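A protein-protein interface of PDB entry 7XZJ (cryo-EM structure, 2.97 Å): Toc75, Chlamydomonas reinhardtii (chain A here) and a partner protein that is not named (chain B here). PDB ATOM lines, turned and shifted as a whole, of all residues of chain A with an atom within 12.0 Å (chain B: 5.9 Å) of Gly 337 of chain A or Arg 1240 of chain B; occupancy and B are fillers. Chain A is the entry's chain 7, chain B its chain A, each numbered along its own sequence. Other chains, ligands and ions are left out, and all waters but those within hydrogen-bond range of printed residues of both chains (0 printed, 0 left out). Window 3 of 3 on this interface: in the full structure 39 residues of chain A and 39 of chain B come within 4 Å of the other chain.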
ATOM      1  N   PRO A 333      26.486  -4.656 -32.961  1.00  0.00           N
ATOM      2  CA  PRO A 333      26.152  -3.827 -31.806  1.00  0.00           C
ATOM      3  C   PRO A 333      26.907  -4.298 -30.556  1.00  0.00           C
ATOM      4  O   PRO A 333      26.658  -5.404 -30.117  1.00  0.00           O
ATOM      5  CB  PRO A 333      24.652  -4.076 -31.594  1.00  0.00           C
ATOM      6  CG  PRO A 333      24.205  -4.880 -32.800  1.00  0.00           C
ATOM      7  CD  PRO A 333      25.438  -5.623 -33.263  1.00  0.00           C
ATOM      8  N   LYS A 334      27.794  -3.457 -30.014  1.00  0.00           N
ATOM      9  CA  LYS A 334      28.599  -3.868 -28.833  1.00  0.00           C
ATOM     10  C   LYS A 334      27.689  -3.857 -27.604  1.00  0.00           C
ATOM     11  O   LYS A 334      26.685  -3.122 -27.632  1.00  0.00           O
ATOM     12  CB  LYS A 334      29.821  -2.965 -28.651  1.00  0.00           C
ATOM     13  CG  LYS A 334      30.936  -3.173 -29.667  1.00  0.00           C
ATOM     14  CD  LYS A 334      32.240  -2.537 -29.243  1.00  0.00           C
ATOM     15  CE  LYS A 334      33.387  -2.859 -30.176  1.00  0.00           C
ATOM     16  NZ  LYS A 334      33.148  -2.327 -31.536  1.00  0.00           N
ATOM     17  N   LEU A 335      28.021  -4.640 -26.576  1.00  0.00           N
ATOM     18  CA  LEU A 335      27.155  -4.733 -25.407  1.00  0.00           C
ATOM     19  C   LEU A 335      27.869  -4.165 -24.186  1.00  0.00           C
ATOM     20  O   LEU A 335      28.949  -4.640 -23.813  1.00  0.00           O
ATOM     21  CB  LEU A 335      26.734  -6.181 -25.159  1.00  0.00           C
ATOM     22  CG  LEU A 335      25.646  -6.387 -24.104  1.00  0.00           C
ATOM     23  CD1 LEU A 335      24.482  -5.439 -24.339  1.00  0.00           C
ATOM     24  CD2 LEU A 335      25.166  -7.826 -24.119  1.00  0.00           C
ATOM     25  N   THR A 336      27.262  -3.154 -23.569  1.00  0.00           N
ATOM     26  CA  THR A 336      27.767  -2.509 -22.364  1.00  0.00           C
ATOM     27  C   THR A 336      26.638  -1.678 -21.775  1.00  0.00           C
ATOM     28  O   THR A 336      25.845  -1.099 -22.520  1.00  0.00           O
ATOM     29  CB  THR A 336      28.986  -1.619 -22.659  1.00  0.00           C
ATOM     30  OG1 THR A 336      29.988  -2.374 -23.350  1.00  0.00           O
ATOM     31  CG2 THR A 336      29.584  -1.090 -21.368  1.00  0.00           C
ATOM     32  N   GLY A 337      26.565  -1.630 -20.448  1.00  0.00           N
ATOM     33  CA  GLY A 337      25.514  -0.884 -19.784  1.00  0.00           C
ATOM     34  C   GLY A 337      25.804   0.600 -19.680  1.00  0.00           C
ATOM     35  O   GLY A 337      26.111   1.104 -18.596  1.00  0.00           O
ATOM     36  N   ASP A 338      25.716   1.314 -20.803  1.00  0.00           N
ATOM     37  CA  ASP A 338      25.997   2.740 -20.836  1.00  0.00           C
ATOM     38  C   ASP A 338      24.819   3.588 -21.293  1.00  0.00           C
ATOM     39  O   ASP A 338      24.979   4.806 -21.438  1.00  0.00           O
ATOM     40  CB  ASP A 338      27.199   3.026 -21.746  1.00  0.00           C
ATOM     41  CG  ASP A 338      28.467   2.370 -21.253  1.00  0.00           C
ATOM     42  OD1 ASP A 338      28.555   2.074 -20.044  1.00  0.00           O
ATOM     43  OD2 ASP A 338      29.377   2.149 -22.078  1.00  0.00           O
ATOM     44  N   SER A 339      23.653   2.986 -21.531  1.00  0.00           N
ATOM     45  CA  SER A 339      22.492   3.686 -22.084  1.00  0.00           C
ATOM     46  C   SER A 339      22.816   4.310 -23.440  1.00  0.00           C
ATOM     47  O   SER A 339      22.186   5.282 -23.861  1.00  0.00           O
ATOM     48  CB  SER A 339      21.952   4.743 -21.116  1.00  0.00           C
ATOM     49  OG  SER A 339      20.679   5.207 -21.522  1.00  0.00           O
ATOM     50  N   GLU A 340      23.802   3.742 -24.127  1.00  0.00           N
ATOM     51  CA  GLU A 340      24.227   4.164 -25.454  1.00  0.00           C
ATOM     52  C   GLU A 340      25.081   3.044 -26.026  1.00  0.00           C
ATOM     53  O   GLU A 340      25.629   2.224 -25.282  1.00  0.00           O
ATOM     54  CB  GLU A 340      24.999   5.490 -25.417  1.00  0.00           C
ATOM     55  CG  GLU A 340      26.277   5.465 -24.591  1.00  0.00           C
ATOM     56  CD  GLU A 340      27.491   5.050 -25.397  1.00  0.00           C
ATOM     57  OE1 GLU A 340      27.416   5.082 -26.643  1.00  0.00           O
ATOM     58  OE2 GLU A 340      28.518   4.688 -24.785  1.00  0.00           O
ATOM     59  N   LEU A 341      25.196   3.017 -27.349  1.00  0.00           N
ATOM     60  CA  LEU A 341      25.803   1.886 -28.032  1.00  0.00           C
ATOM     61  C   LEU A 341      26.851   2.355 -29.031  1.00  0.00           C
ATOM     62  O   LEU A 341      26.769   3.457 -29.580  1.00  0.00           O
ATOM     63  CB  LEU A 341      24.744   1.044 -28.755  1.00  0.00           C
ATOM     64  CG  LEU A 341      23.703   0.366 -27.864  1.00  0.00           C
ATOM     65  CD1 LEU A 341      22.546  -0.147 -28.699  1.00  0.00           C
ATOM     66  CD2 LEU A 341      24.339  -0.767 -27.076  1.00  0.00           C
ATOM     67  N   GLU A 342      27.842   1.492 -29.261  1.00  0.00           N
ATOM     68  CA  GLU A 342      28.871   1.775 -30.291  1.00  0.00           C
ATOM     69  C   GLU A 342      28.809   0.592 -31.259  1.00  0.00           C
ATOM     70  O   GLU A 342      28.716  -0.548 -30.774  1.00  0.00           O
ATOM     71  CB  GLU A 342      30.249   1.902 -29.640  1.00  0.00           C
ATOM     72  CG  GLU A 342      31.304   2.514 -30.547  1.00  0.00           C
ATOM     73  CD  GLU A 342      31.968   1.563 -31.529  1.00  0.00           C
ATOM     74  OE1 GLU A 342      31.981   0.348 -31.258  1.00  0.00           O
ATOM     75  OE2 GLU A 342      32.464   2.041 -32.568  1.00  0.00           O
ATOM     76  N   GLN A 414      23.903 -12.800 -31.560  1.00  0.00           N
ATOM     77  CA  GLN A 414      25.101 -13.244 -30.793  1.00  0.00           C
ATOM     78  C   GLN A 414      24.681 -14.393 -29.872  1.00  0.00           C
ATOM     79  O   GLN A 414      24.102 -14.112 -28.806  1.00  0.00           O
ATOM     80  CB  GLN A 414      25.724 -12.067 -30.041  1.00  0.00           C
ATOM     81  CG  GLN A 414      26.092 -10.899 -30.945  1.00  0.00           C
ATOM     82  CD  GLN A 414      26.645  -9.720 -30.185  1.00  0.00           C
ATOM     83  OE1 GLN A 414      27.059  -9.836 -29.034  1.00  0.00           O
ATOM     84  NE2 GLN A 414      26.660  -8.565 -30.832  1.00  0.00           N
ATOM     85  N   TRP B1235      23.730  10.543 -11.602  1.00  0.00           N
ATOM     86  CA  TRP B1235      22.311  10.235 -11.474  1.00  0.00           C
ATOM     87  C   TRP B1235      22.007   8.808 -11.909  1.00  0.00           C
ATOM     88  O   TRP B1235      21.192   8.126 -11.283  1.00  0.00           O
ATOM     89  CB  TRP B1235      21.475  11.217 -12.285  1.00  0.00           C
ATOM     90  CG  TRP B1235      20.021  10.873 -12.249  1.00  0.00           C
ATOM     91  CD1 TRP B1235      19.115  11.255 -11.307  1.00  0.00           C
ATOM     92  CD2 TRP B1235      19.309  10.057 -13.185  1.00  0.00           C
ATOM     93  NE1 TRP B1235      17.878  10.736 -11.602  1.00  0.00           N
ATOM     94  CE2 TRP B1235      17.971   9.997 -12.751  1.00  0.00           C
ATOM     95  CE3 TRP B1235      19.670   9.377 -14.349  1.00  0.00           C
ATOM     96  CZ2 TRP B1235      16.995   9.284 -13.439  1.00  0.00           C
ATOM     97  CZ3 TRP B1235      18.700   8.670 -15.031  1.00  0.00           C
ATOM     98  CH2 TRP B1235      17.379   8.630 -14.574  1.00  0.00           C
ATOM     99  N   ARG B1236      22.622   8.348 -12.997  1.00  0.00           N
ATOM    100  CA  ARG B1236      22.410   6.969 -13.433  1.00  0.00           C
ATOM    101  C   ARG B1236      22.939   5.978 -12.403  1.00  0.00           C
ATOM    102  O   ARG B1236      22.304   4.950 -12.122  1.00  0.00           O
ATOM    103  CB  ARG B1236      23.082   6.741 -14.786  1.00  0.00           C
ATOM    104  CG  ARG B1236      22.511   7.587 -15.911  1.00  0.00           C
ATOM    105  CD  ARG B1236      23.268   7.375 -17.210  1.00  0.00           C
ATOM    106  NE  ARG B1236      22.614   8.046 -18.325  1.00  0.00           N
ATOM    107  CZ  ARG B1236      23.103   8.105 -19.559  1.00  0.00           C
ATOM    108  NH1 ARG B1236      24.263   7.552 -19.870  1.00  0.00           N
ATOM    109  NH2 ARG B1236      22.410   8.738 -20.499  1.00  0.00           N
ATOM    110  N   THR B1237      24.109   6.270 -11.837  1.00  0.00           N
ATOM    111  CA  THR B1237      24.667   5.388 -10.821  1.00  0.00           C
ATOM    112  C   THR B1237      23.749   5.307  -9.607  1.00  0.00           C
ATOM    113  O   THR B1237      23.567   4.230  -9.027  1.00  0.00           O
ATOM    114  CB  THR B1237      26.058   5.867 -10.414  1.00  0.00           C
ATOM    115  OG1 THR B1237      26.834   6.130 -11.588  1.00  0.00           O
ATOM    116  CG2 THR B1237      26.761   4.804  -9.589  1.00  0.00           C
ATOM    117  N   LYS B1238      23.172   6.440  -9.199  1.00  0.00           N
ATOM    118  CA  LYS B1238      22.187   6.419  -8.120  1.00  0.00           C
ATOM    119  C   LYS B1238      20.921   5.672  -8.535  1.00  0.00           C
ATOM    120  O   LYS B1238      20.307   4.973  -7.720  1.00  0.00           O
ATOM    121  CB  LYS B1238      21.845   7.845  -7.692  1.00  0.00           C
ATOM    122  CG  LYS B1238      20.838   7.921  -6.561  1.00  0.00           C
ATOM    123  CD  LYS B1238      20.351   9.341  -6.349  1.00  0.00           C
ATOM    124  CE  LYS B1238      19.705   9.897  -7.606  1.00  0.00           C
ATOM    125  NZ  LYS B1238      19.216  11.287  -7.401  1.00  0.00           N
ATOM    126  N   GLN B1239      20.507   5.827  -9.794  1.00  0.00           N
ATOM    127  CA  GLN B1239      19.288   5.183 -10.271  1.00  0.00           C
ATOM    128  C   GLN B1239      19.409   3.669 -10.202  1.00  0.00           C
ATOM    129  O   GLN B1239      18.424   2.969  -9.931  1.00  0.00           O
ATOM    130  CB  GLN B1239      18.986   5.635 -11.699  1.00  0.00           C
ATOM    131  CG  GLN B1239      17.730   5.022 -12.294  1.00  0.00           C
ATOM    132  CD  GLN B1239      16.460   5.565 -11.670  1.00  0.00           C
ATOM    133  OE1 GLN B1239      16.456   6.646 -11.084  1.00  0.00           O
ATOM    134  NE2 GLN B1239      15.371   4.816 -11.797  1.00  0.00           N
ATOM    135  N   ARG B1240      20.610   3.146 -10.456  1.00  0.00           N
ATOM    136  CA  ARG B1240      20.822   1.708 -10.306  1.00  0.00           C
ATOM    137  C   ARG B1240      20.459   1.244  -8.900  1.00  0.00           C
ATOM    138  O   ARG B1240      19.801   0.212  -8.728  1.00  0.00           O
ATOM    139  CB  ARG B1240      22.270   1.345 -10.624  1.00  0.00           C
ATOM    140  CG  ARG B1240      22.575   1.205 -12.099  1.00  0.00           C
ATOM    141  CD  ARG B1240      23.855   0.416 -12.298  1.00  0.00           C
ATOM    142  NE  ARG B1240      24.237   0.330 -13.698  1.00  0.00           N
ATOM    143  CZ  ARG B1240      25.232  -0.423 -14.158  1.00  0.00           C
ATOM    144  NH1 ARG B1240      25.952  -1.183 -13.350  1.00  0.00           N
ATOM    145  NH2 ARG B1240      25.505  -0.413 -15.457  1.00  0.00           N
ATOM    146  N   VAL B1241      20.817   2.035  -7.887  1.00  0.00           N
ATOM    147  CA  VAL B1241      20.482   1.671  -6.478  1.00  0.00           C
ATOM    148  C   VAL B1241      18.963   1.719  -6.283  1.00  0.00           C
ATOM    149  O   VAL B1241      18.424   0.799  -5.637  1.00  0.00           O
ATOM    150  CB  VAL B1241      21.208   2.591  -5.483  1.00  0.00           C
ATOM    151  CG1 VAL B1241      21.061   2.106  -4.050  1.00  0.00           C
ATOM    152  CG2 VAL B1241      22.672   2.723  -5.851  1.00  0.00           C
ATOM    153  N   ILE B1242      18.300   2.743  -6.827  1.00  0.00           N
ATOM    154  CA  ILE B1242      16.829   2.911  -6.623  1.00  0.00           C
ATOM    155  C   ILE B1242      16.086   1.717  -7.233  1.00  0.00           C
ATOM    156  O   ILE B1242      15.130   1.236  -6.596  1.00  0.00           O
ATOM    157  CB  ILE B1242      16.352   4.250  -7.221  1.00  0.00           C
ATOM    158  CG1 ILE B1242      17.177   5.428  -6.698  1.00  0.00           C
ATOM    159  CG2 ILE B1242      14.865   4.458  -6.983  1.00  0.00           C
ATOM    160  CD1 ILE B1242      16.805   6.758  -7.310  1.00  0.00           C
ATOM    161  N   THR B1243      16.511   1.251  -8.410  1.00  0.00           N
ATOM    162  CA  THR B1243      15.783   0.152  -9.101  1.00  0.00           C
ATOM    163  C   THR B1243      15.827  -1.135  -8.272  1.00  0.00           C
ATOM    164  O   THR B1243      15.015  -2.035  -8.558  1.00  0.00           O
ATOM    165  CB  THR B1243      16.345  -0.097 -10.506  1.00  0.00           C
ATOM    166  OG1 THR B1243      17.716  -0.477 -10.385  1.00  0.00           O
ATOM    167  CG2 THR B1243      16.225   1.109 -11.411  1.00  0.00           C
ATOM    168  N   LYS B1244      16.729  -1.225  -7.289  1.00  0.00           N
ATOM    169  CA  LYS B1244      16.878  -2.494  -6.526  1.00  0.00           C
ATOM    170  C   LYS B1244      16.249  -2.356  -5.139  1.00  0.00           C
ATOM    171  O   LYS B1244      16.530  -3.216  -4.291  1.00  0.00           O
ATOM    172  CB  LYS B1244      18.356  -2.860  -6.376  1.00  0.00           C
ATOM    173  CG  LYS B1244      19.137  -2.988  -7.675  1.00  0.00           C
ATOM    174  CD  LYS B1244      20.492  -3.623  -7.470  1.00  0.00           C
ATOM    175  CE  LYS B1244      21.233  -3.049  -6.283  1.00  0.00           C
ATOM    176  NZ  LYS B1244      21.620  -1.635  -6.506  1.00  0.00           N
ATOM    177  N   HIS B1444      20.838  -6.128 -23.098  1.00  0.00           N
ATOM    178  CA  HIS B1444      21.248  -4.770 -22.769  1.00  0.00           C
ATOM    179  C   HIS B1444      20.585  -4.291 -21.486  1.00  0.00           C
ATOM    180  O   HIS B1444      21.203  -3.575 -20.694  1.00  0.00           O
ATOM    181  CB  HIS B1444      20.927  -3.832 -23.931  1.00  0.00           C
ATOM    182  CG  HIS B1444      21.565  -2.483 -23.810  1.00  0.00           C
ATOM    183  ND1 HIS B1444      20.869  -1.363 -23.411  1.00  0.00           N
ATOM    184  CD2 HIS B1444      22.837  -2.076 -24.032  1.00  0.00           C
ATOM    185  CE1 HIS B1444      21.683  -0.324 -23.393  1.00  0.00           C
ATOM    186  NE2 HIS B1444      22.884  -0.729 -23.767  1.00  0.00           N
ATOM    187  N   TYR B1447      22.293  -5.675 -18.637  1.00  0.00           N
ATOM    188  CA  TYR B1447      23.558  -4.987 -18.408  1.00  0.00           C
ATOM    189  C   TYR B1447      23.383  -3.622 -17.742  1.00  0.00           C
ATOM    190  O   TYR B1447      24.096  -3.303 -16.787  1.00  0.00           O
ATOM    191  CB  TYR B1447      24.313  -4.836 -19.730  1.00  0.00           C
ATOM    192  CG  TYR B1447      25.312  -5.939 -19.980  1.00  0.00           C
ATOM    193  CD1 TYR B1447      24.900  -7.193 -20.407  1.00  0.00           C
ATOM    194  CD2 TYR B1447      26.668  -5.727 -19.788  1.00  0.00           C
ATOM    195  CE1 TYR B1447      25.812  -8.201 -20.633  1.00  0.00           C
ATOM    196  CE2 TYR B1447      27.586  -6.729 -20.013  1.00  0.00           C
ATOM    197  CZ  TYR B1447      27.153  -7.964 -20.435  1.00  0.00           C
ATOM    198  OH  TYR B1447      28.066  -8.966 -20.660  1.00  0.00           O
ATOM    199  N   ARG B1448      22.461  -2.795 -18.240  1.00  0.00           N
ATOM    200  CA  ARG B1448      22.361  -1.421 -17.749  1.00  0.00           C
ATOM    201  C   ARG B1448      21.753  -1.359 -16.351  1.00  0.00           C
ATOM    202  O   ARG B1448      22.164  -0.535 -15.527  1.00  0.00           O
ATOM    203  CB  ARG B1448      21.571  -0.558 -18.737  1.00  0.00           C
ATOM    204  CG  ARG B1448      20.088  -0.860 -18.866  1.00  0.00           C
ATOM    205  CD  ARG B1448      19.489  -0.071 -20.022  1.00  0.00           C
ATOM    206  NE  ARG B1448      18.036  -0.006 -19.953  1.00  0.00           N
ATOM    207  CZ  ARG B1448      17.357   1.005 -19.425  1.00  0.00           C
ATOM    208  NH1 ARG B1448      17.972   2.061 -18.918  1.00  0.00           N
ATOM    209  NH2 ARG B1448      16.029   0.958 -19.408  1.00  0.00           N
ATOM    210  N   LYS B1449      20.770  -2.217 -16.068  1.00  0.00           N
ATOM    211  CA  LYS B1449      20.132  -2.288 -14.748  1.00  0.00           C
ATOM    212  C   LYS B1449      19.539  -0.945 -14.323  1.00  0.00           C
ATOM    213  O   LYS B1449      19.669  -0.529 -13.171  1.00  0.00           O
ATOM    214  CB  LYS B1449      21.111  -2.786 -13.681  1.00  0.00           C
ATOM    215  CG  LYS B1449      21.847  -4.072 -14.014  1.00  0.00           C
ATOM    216  CD  LYS B1449      22.886  -4.357 -12.937  1.00  0.00           C
ATOM    217  CE  LYS B1449      23.715  -5.587 -13.252  1.00  0.00           C
ATOM    218  NZ  LYS B1449      24.786  -5.792 -12.238  1.00  0.00           N
ATOM    219  N   ARG B1450      18.877  -0.260 -15.248  1.00  0.00           N
ATOM    220  CA  ARG B1450      18.317   1.051 -14.960  1.00  0.00           C
ATOM    221  C   ARG B1450      16.872   1.134 -15.430  1.00  0.00           C
ATOM    222  O   ARG B1450      16.430   0.389 -16.307  1.00  0.00           O
ATOM    223  CB  ARG B1450      19.133   2.175 -15.610  1.00  0.00           C
ATOM    224  CG  ARG B1450      20.415   2.514 -14.872  1.00  0.00           C
ATOM    225  CD  ARG B1450      21.113   3.712 -15.486  1.00  0.00           C
ATOM    226  NE  ARG B1450      21.614   3.427 -16.823  1.00  0.00           N
ATOM    227  CZ  ARG B1450      22.832   2.966 -17.083  1.00  0.00           C
ATOM    228  NH1 ARG B1450      23.702   2.727 -16.116  1.00  0.00           N
ATOM    229  NH2 ARG B1450      23.184   2.742 -18.344  1.00  0.00           N
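The backbone carbonyl oxygen (O) of Gly 337 of chain A sits at hydrogen-bond distance from the guanidinium group (NH2) of Arg 1450 of chain B (3.4 Å). The backbone carbonyl oxygen (O) of Thr 336 of chain A lies within hydrogen-bond range of a ring nitrogen (NE2) of His 1444 of chain B, 3.2 Å away. N of Ser 339 of chain A lies close to NH2 of Arg 1450 of chain B (3.2 Å). The backbone carbonyl oxygen of Asp 338 of chain A sits at hydrogen-bond distance from the guanidinium group of Arg 1236 of chain B (3.2 Å).
The guanidinium group (NE) of Arg 1240 of chain B lies within hydrogen-bond range of the backbone carbonyl oxygen (O) of Arg 1448 of chain B, at 2.9 Å. The backbone carbonyl oxygen (O) of Tyr 1447 of chain B is in hydrogen-bond range of the guanidinium group (NH2) of Arg 1240 of chain B (3.5 Å). O of Arg 1240 of chain B sits at hydrogen-bond distance from NZ of Lys 1244 of chain B (3.4 Å). The backbone carbonyl oxygen of Arg 1240 of chain B is in hydrogen-bond range of the side-chain hydroxyl of Thr 1243 of chain B (2.8 Å). The backbone carbonyl oxygen of Arg 1450 of chain B lies within hydrogen-bond range of the guanidinium group of Arg 1448 of chain B.
Among the printed residues, merely in contact across the chains: Leu 335 of chain A with His 1444 of chain B (3.7 Å), Leu 335 of chain A with Tyr 1447 of chain B (3.6 Å), Gly 337 of chain A with Arg 1240 of chain B (3.5 Å), Gly 337 of chain A with Tyr 1447 of chain B (3.98 Å), Gly 337 of chain A with Arg 1448 of chain B (3.8 Å), Asp 338 of chain A with Arg 1450 of chain B (3.5 Å), Ser 339 of chain A with Arg 1236 of chain B (3.8 Å) and Leu 341 of chain A with His 1444 of chain B (3.6 Å).
Arg 1240 of chain B touches just one residue of chain A: Gly 337. No residue of chain A comes within 4 Å of Thr 1237 of chain B. No residue of chain A comes within 4 Å of Gln 1239 of chain B. No residue of chain A comes within 4 Å of Val 1241 of chain B. No residue of chain A comes within 4 Å of Ile 1242 of chain B. No residue of chain A comes within 4 Å of Lys 1244 of chain B. No residue of chain A comes within 4 Å of Lys 1449 of chain B. Arg 1450 of chain B touches just these residues of chain A: Gly 337 (3.4 Å), Asp 338 (3.5 Å) and Ser 339 (3.2 Å). Printed residues of chain B within 4 Å of Leu 335 of chain A: His 1444 and Tyr 1447. Of the printed residues of chain A, Arg 1448 of chain B touches Gly 337 (3.8 Å). Glu 342 of chain A touches none of the printed residues of chain B. The nearest printed residue of chain B that does not touch Gly 337 of chain A is His 1444 of chain B (4.8 Å).
Of the 15 printed residues of chain B, 6 touch a printed residue of chain A. Hydrophobic or aromatic side chains of chain B within 4 Å of the printed part of chain A: His 1444 and Tyr 1447. Of the 11 printed residues of chain A, 6 touch a printed residue of chain B. Printed residues of chain A that touch a printed residue of chain B: Leu 335, Thr 336, Gly 337, Asp 338, Ser 339 and Leu 341. Hydrophobic or aromatic side chains of chain A that line the printed part of chain B: Leu 335 and Leu 341.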
